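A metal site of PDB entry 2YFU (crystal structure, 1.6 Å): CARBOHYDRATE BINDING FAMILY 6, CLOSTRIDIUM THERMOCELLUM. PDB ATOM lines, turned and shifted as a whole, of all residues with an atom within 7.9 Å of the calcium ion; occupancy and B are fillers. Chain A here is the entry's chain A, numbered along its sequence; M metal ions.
N of Asn 34 is in hydrogen-bond range of OD1 of Asp 32 (2.9 Å). OE2 of Glu 133 lies within hydrogen-bond range of N of Gly 31, at 2.7 Å. The backbone carbonyl oxygen of Glu 133 sits at hydrogen-bond distance from the backbone NH of Cys 65 (2.9 Å). N of Ala 132 sits at hydrogen-bond distance from O of Cys 65, at 2.7 Å.
Of the 19 residues printed, 6 come within 4 Å of the calcium ion.
The calcium ion is bound by the backbone carbonyl oxygen of Lys 27, the backbone carbonyl oxygen of Asp 32, the side-chain carboxylate of Glu 133, the backbone carbonyl oxygen of Ala 132, the backbone carbonyl oxygen of Thr 35, the side-chain hydroxyl of Thr 35 and the side-chain carboxylate of Asp 30.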
ATOM      1  N   THR A  24     -14.251  24.016 -31.309  1.00  0.00           N
ATOM      2  CA  THR A  24     -13.256  24.255 -30.242  1.00  0.00           C
ATOM      3  C   THR A  24     -13.574  23.404 -29.009  1.00  0.00           C
ATOM      4  O   THR A  24     -14.600  22.673 -28.936  1.00  0.00           O
ATOM      5  CB  THR A  24     -13.277  25.697 -29.779  1.00  0.00           C
ATOM      6  OG1 THR A  24     -14.563  25.981 -29.191  1.00  0.00           O
ATOM      7  CG2 THR A  24     -13.022  26.665 -30.980  1.00  0.00           C
ATOM      8  N   ILE A  25     -12.711  23.516 -28.013  1.00  0.00           N
ATOM      9  CA  ILE A  25     -12.909  22.799 -26.738  1.00  0.00           C
ATOM     10  C   ILE A  25     -14.267  23.083 -26.099  1.00  0.00           C
ATOM     11  O   ILE A  25     -14.788  22.253 -25.363  1.00  0.00           O
ATOM     12  CB  ILE A  25     -11.748  23.073 -25.721  1.00  0.00           C
ATOM     13  CG1 ILE A  25     -11.590  24.579 -25.468  1.00  0.00           C
ATOM     14  CG2 ILE A  25     -10.449  22.430 -26.278  1.00  0.00           C
ATOM     15  CD1 ILE A  25     -10.421  24.939 -24.480  1.00  0.00           C
ATOM     16  N   HIS A  26     -14.841  24.263 -26.387  1.00  0.00           N
ATOM     17  CA  HIS A  26     -16.113  24.612 -25.787  1.00  0.00           C
ATOM     18  C   HIS A  26     -17.254  23.687 -26.208  1.00  0.00           C
ATOM     19  O   HIS A  26     -18.245  23.569 -25.462  1.00  0.00           O
ATOM     20  CB  HIS A  26     -16.442  26.075 -26.101  1.00  0.00           C
ATOM     21  CG  HIS A  26     -15.500  27.013 -25.428  1.00  0.00           C
ATOM     22  ND1 HIS A  26     -15.668  27.422 -24.117  1.00  0.00           N
ATOM     23  CD2 HIS A  26     -14.301  27.519 -25.837  1.00  0.00           C
ATOM     24  CE1 HIS A  26     -14.653  28.202 -23.778  1.00  0.00           C
ATOM     25  NE2 HIS A  26     -13.802  28.258 -24.795  1.00  0.00           N
ATOM     26  N   LYS A  27     -17.097  23.012 -27.345  1.00  0.00           N
ATOM     27  CA  LYS A  27     -18.142  22.072 -27.808  1.00  0.00           C
ATOM     28  C   LYS A  27     -18.265  20.877 -26.904  1.00  0.00           C
ATOM     29  O   LYS A  27     -19.273  20.154 -26.981  1.00  0.00           O
ATOM     30  CB  LYS A  27     -17.847  21.575 -29.232  1.00  0.00           C
ATOM     31  CG  LYS A  27     -17.748  22.664 -30.288  1.00  0.00           C
ATOM     32  CD  LYS A  27     -18.985  23.576 -30.287  1.00  0.00           C
ATOM     33  CE  LYS A  27     -18.764  24.635 -31.375  1.00  0.00           C
ATOM     34  NZ  LYS A  27     -19.707  25.807 -31.180  1.00  0.00           N
ATOM     35  N   ALA A  28     -17.283  20.620 -26.038  1.00  0.00           N
ATOM     36  CA  ALA A  28     -17.398  19.469 -25.123  1.00  0.00           C
ATOM     37  C   ALA A  28     -18.171  19.780 -23.858  1.00  0.00           C
ATOM     38  O   ALA A  28     -18.333  18.886 -22.987  1.00  0.00           O
ATOM     39  CB  ALA A  28     -15.962  18.942 -24.758  1.00  0.00           C
ATOM     40  N   PHE A  29     -18.667  21.021 -23.726  1.00  0.00           N
ATOM     41  CA  PHE A  29     -19.332  21.433 -22.480  1.00  0.00           C
ATOM     42  C   PHE A  29     -20.698  22.048 -22.724  1.00  0.00           C
ATOM     43  O   PHE A  29     -21.268  22.681 -21.814  1.00  0.00           O
ATOM     44  CB  PHE A  29     -18.444  22.417 -21.685  1.00  0.00           C
ATOM     45  CG  PHE A  29     -17.076  21.873 -21.380  1.00  0.00           C
ATOM     46  CD1 PHE A  29     -16.882  21.078 -20.229  1.00  0.00           C
ATOM     47  CD2 PHE A  29     -16.003  22.109 -22.234  1.00  0.00           C
ATOM     48  CE1 PHE A  29     -15.610  20.582 -19.922  1.00  0.00           C
ATOM     49  CE2 PHE A  29     -14.717  21.596 -21.947  1.00  0.00           C
ATOM     50  CZ  PHE A  29     -14.520  20.832 -20.796  1.00  0.00           C
ATOM     51  N   ASP A  30     -21.236  21.841 -23.914  1.00  0.00           N
ATOM     52  CA  ASP A  30     -22.442  22.555 -24.347  1.00  0.00           C
ATOM     53  C   ASP A  30     -23.721  21.764 -24.154  1.00  0.00           C
ATOM     54  O   ASP A  30     -24.797  22.302 -24.462  1.00  0.00           O
ATOM     55  CB  ASP A  30     -22.346  23.032 -25.798  1.00  0.00           C
ATOM     56  CG  ASP A  30     -22.157  21.927 -26.795  1.00  0.00           C
ATOM     57  OD1 ASP A  30     -22.142  20.751 -26.402  1.00  0.00           O
ATOM     58  OD2 ASP A  30     -22.003  22.267 -27.989  1.00  0.00           O
ATOM     59  N   GLY A  31     -23.603  20.551 -23.642  1.00  0.00           N
ATOM     60  CA  GLY A  31     -24.824  19.702 -23.431  1.00  0.00           C
ATOM     61  C   GLY A  31     -25.321  18.989 -24.663  1.00  0.00           C
ATOM     62  O   GLY A  31     -26.322  18.244 -24.571  1.00  0.00           O
ATOM     63  N   ASP A  32     -24.666  19.162 -25.805  1.00  0.00           N
ATOM     64  CA  ASP A  32     -25.130  18.521 -27.046  1.00  0.00           C
ATOM     65  C   ASP A  32     -24.186  17.384 -27.410  1.00  0.00           C
ATOM     66  O   ASP A  32     -22.982  17.639 -27.645  1.00  0.00           O
ATOM     67  CB  ASP A  32     -25.173  19.563 -28.182  1.00  0.00           C
ATOM     68  CG  ASP A  32     -25.836  19.045 -29.438  1.00  0.00           C
ATOM     69  OD1 ASP A  32     -26.135  17.838 -29.513  1.00  0.00           O
ATOM     70  OD2 ASP A  32     -26.068  19.865 -30.348  1.00  0.00           O
ATOM     71  N   LEU A  33     -24.681  16.135 -27.464  1.00  0.00           N
ATOM     72  CA  LEU A  33     -23.773  15.019 -27.788  1.00  0.00           C
ATOM     73  C   LEU A  33     -23.429  14.993 -29.272  1.00  0.00           C
ATOM     74  O   LEU A  33     -22.554  14.233 -29.687  1.00  0.00           O
ATOM     75  CB  LEU A  33     -24.376  13.677 -27.343  1.00  0.00           C
ATOM     76  CG  LEU A  33     -24.831  13.612 -25.890  1.00  0.00           C
ATOM     77  CD1 LEU A  33     -25.280  12.159 -25.569  1.00  0.00           C
ATOM     78  CD2 LEU A  33     -23.709  14.073 -24.909  1.00  0.00           C
ATOM     79  N   ASN A  34     -24.118  15.823 -30.057  1.00  0.00           N
ATOM     80  CA  ASN A  34     -23.817  15.918 -31.488  1.00  0.00           C
ATOM     81  C   ASN A  34     -22.702  16.897 -31.826  1.00  0.00           C
ATOM     82  O   ASN A  34     -22.257  16.921 -32.980  1.00  0.00           O
ATOM     83  CB  ASN A  34     -25.075  16.398 -32.226  1.00  0.00           C
ATOM     84  CG  ASN A  34     -26.242  15.460 -32.007  1.00  0.00           C
ATOM     85  OD1 ASN A  34     -27.237  15.820 -31.340  1.00  0.00           O
ATOM     86  ND2 ASN A  34     -26.125  14.241 -32.506  1.00  0.00           N
ATOM     87  N   THR A  35     -22.317  17.753 -30.880  1.00  0.00           N
ATOM     88  CA  THR A  35     -21.231  18.722 -31.127  1.00  0.00           C
ATOM     89  C   THR A  35     -19.997  18.215 -30.420  1.00  0.00           C
ATOM     90  O   THR A  35     -20.097  17.633 -29.332  1.00  0.00           O
ATOM     91  CB  THR A  35     -21.515  20.102 -30.583  1.00  0.00           C
ATOM     92  OG1 THR A  35     -21.730  20.030 -29.182  1.00  0.00           O
ATOM     93  CG2 THR A  35     -22.754  20.740 -31.218  1.00  0.00           C
ATOM     94  N   PHE A  36     -18.827  18.440 -31.045  1.00  0.00           N
ATOM     95  CA  PHE A  36     -17.602  17.812 -30.550  1.00  0.00           C
ATOM     96  C   PHE A  36     -16.433  18.780 -30.689  1.00  0.00           C
ATOM     97  O   PHE A  36     -16.489  19.717 -31.507  1.00  0.00           O
ATOM     98  CB  PHE A  36     -17.290  16.517 -31.333  1.00  0.00           C
ATOM     99  CG  PHE A  36     -17.335  16.709 -32.819  1.00  0.00           C
ATOM    100  CD1 PHE A  36     -16.195  17.124 -33.530  1.00  0.00           C
ATOM    101  CD2 PHE A  36     -18.522  16.533 -33.502  1.00  0.00           C
ATOM    102  CE1 PHE A  36     -16.259  17.349 -34.914  1.00  0.00           C
ATOM    103  CE2 PHE A  36     -18.602  16.743 -34.877  1.00  0.00           C
ATOM    104  CZ  PHE A  36     -17.494  17.160 -35.588  1.00  0.00           C
ATOM    105  N   PHE A  37     -15.394  18.540 -29.893  1.00  0.00           N
ATOM    106  CA  PHE A  37     -14.091  19.203 -30.070  1.00  0.00           C
ATOM    107  C   PHE A  37     -13.317  18.464 -31.164  1.00  0.00           C
ATOM    108  O   PHE A  37     -13.137  17.247 -31.093  1.00  0.00           O
ATOM    109  CB  PHE A  37     -13.333  19.092 -28.739  1.00  0.00           C
ATOM    110  CG  PHE A  37     -11.873  19.556 -28.801  1.00  0.00           C
ATOM    111  CD1 PHE A  37     -11.505  20.727 -29.488  1.00  0.00           C
ATOM    112  CD2 PHE A  37     -10.883  18.799 -28.147  1.00  0.00           C
ATOM    113  CE1 PHE A  37     -10.161  21.159 -29.520  1.00  0.00           C
ATOM    114  CE2 PHE A  37      -9.524  19.214 -28.170  1.00  0.00           C
ATOM    115  CZ  PHE A  37      -9.165  20.384 -28.877  1.00  0.00           C
ATOM    116  N   CYS A  65     -18.635  11.442 -23.714  1.00  0.00           N
ATOM    117  CA  CYS A  65     -19.243  10.876 -24.922  1.00  0.00           C
ATOM    118  C   CYS A  65     -18.243  11.109 -26.046  1.00  0.00           C
ATOM    119  O   CYS A  65     -17.745  12.229 -26.185  1.00  0.00           O
ATOM    120  CB  CYS A  65     -20.529  11.658 -25.233  1.00  0.00           C
ATOM    121  SG  CYS A  65     -21.370  11.069 -26.769  1.00  0.00           S
ATOM    122  N   ILE A 131     -13.736  14.399 -28.792  1.00  0.00           N
ATOM    123  CA  ILE A 131     -14.622  14.083 -27.681  1.00  0.00           C
ATOM    124  C   ILE A 131     -15.843  14.974 -27.890  1.00  0.00           C
ATOM    125  O   ILE A 131     -15.701  16.140 -28.295  1.00  0.00           O
ATOM    126  CB  ILE A 131     -13.920  14.339 -26.301  1.00  0.00           C
ATOM    127  CG1 ILE A 131     -14.845  13.939 -25.142  1.00  0.00           C
ATOM    128  CG2 ILE A 131     -13.375  15.828 -26.182  1.00  0.00           C
ATOM    129  CD1 ILE A 131     -14.100  14.031 -23.776  1.00  0.00           C
ATOM    130  N   ALA A 132     -17.031  14.424 -27.662  1.00  0.00           N
ATOM    131  CA  ALA A 132     -18.256  15.251 -27.852  1.00  0.00           C
ATOM    132  C   ALA A 132     -18.727  15.942 -26.582  1.00  0.00           C
ATOM    133  O   ALA A 132     -19.315  17.019 -26.652  1.00  0.00           O
ATOM    134  CB  ALA A 132     -19.414  14.387 -28.442  1.00  0.00           C
ATOM    135  N   GLU A 133     -18.525  15.315 -25.438  1.00  0.00           N
ATOM    136  CA  GLU A 133     -19.021  15.907 -24.189  1.00  0.00           C
ATOM    137  C   GLU A 133     -18.209  15.359 -23.019  1.00  0.00           C
ATOM    138  O   GLU A 133     -17.802  14.184 -23.029  1.00  0.00           O
ATOM    139  CB  GLU A 133     -20.533  15.561 -24.014  1.00  0.00           C
ATOM    140  CG  GLU A 133     -21.293  16.558 -23.134  1.00  0.00           C
ATOM    141  CD  GLU A 133     -21.452  17.959 -23.741  1.00  0.00           C
ATOM    142  OE1 GLU A 133     -21.465  18.111 -24.987  1.00  0.00           O
ATOM    143  OE2 GLU A 133     -21.637  18.894 -22.937  1.00  0.00           O
ATOM    144  N   LEU A 134     -17.982  16.223 -22.031  1.00  0.00           N
ATOM    145  CA  LEU A 134     -17.106  15.900 -20.896  1.00  0.00           C
ATOM    146  C   LEU A 134     -17.716  16.534 -19.665  1.00  0.00           C
ATOM    147  O   LEU A 134     -18.046  17.730 -19.675  1.00  0.00           O
ATOM    148  CB  LEU A 134     -15.728  16.512 -21.154  1.00  0.00           C
ATOM    149  CG  LEU A 134     -14.728  16.346 -19.986  1.00  0.00           C
ATOM    150  CD1 LEU A 134     -14.536  14.857 -19.662  1.00  0.00           C
ATOM    151  CD2 LEU A 134     -13.415  17.008 -20.433  1.00  0.00           C
HETATM  152 CA    CA M   1     -20.957  18.665 -27.210  1.00  0.00          CA
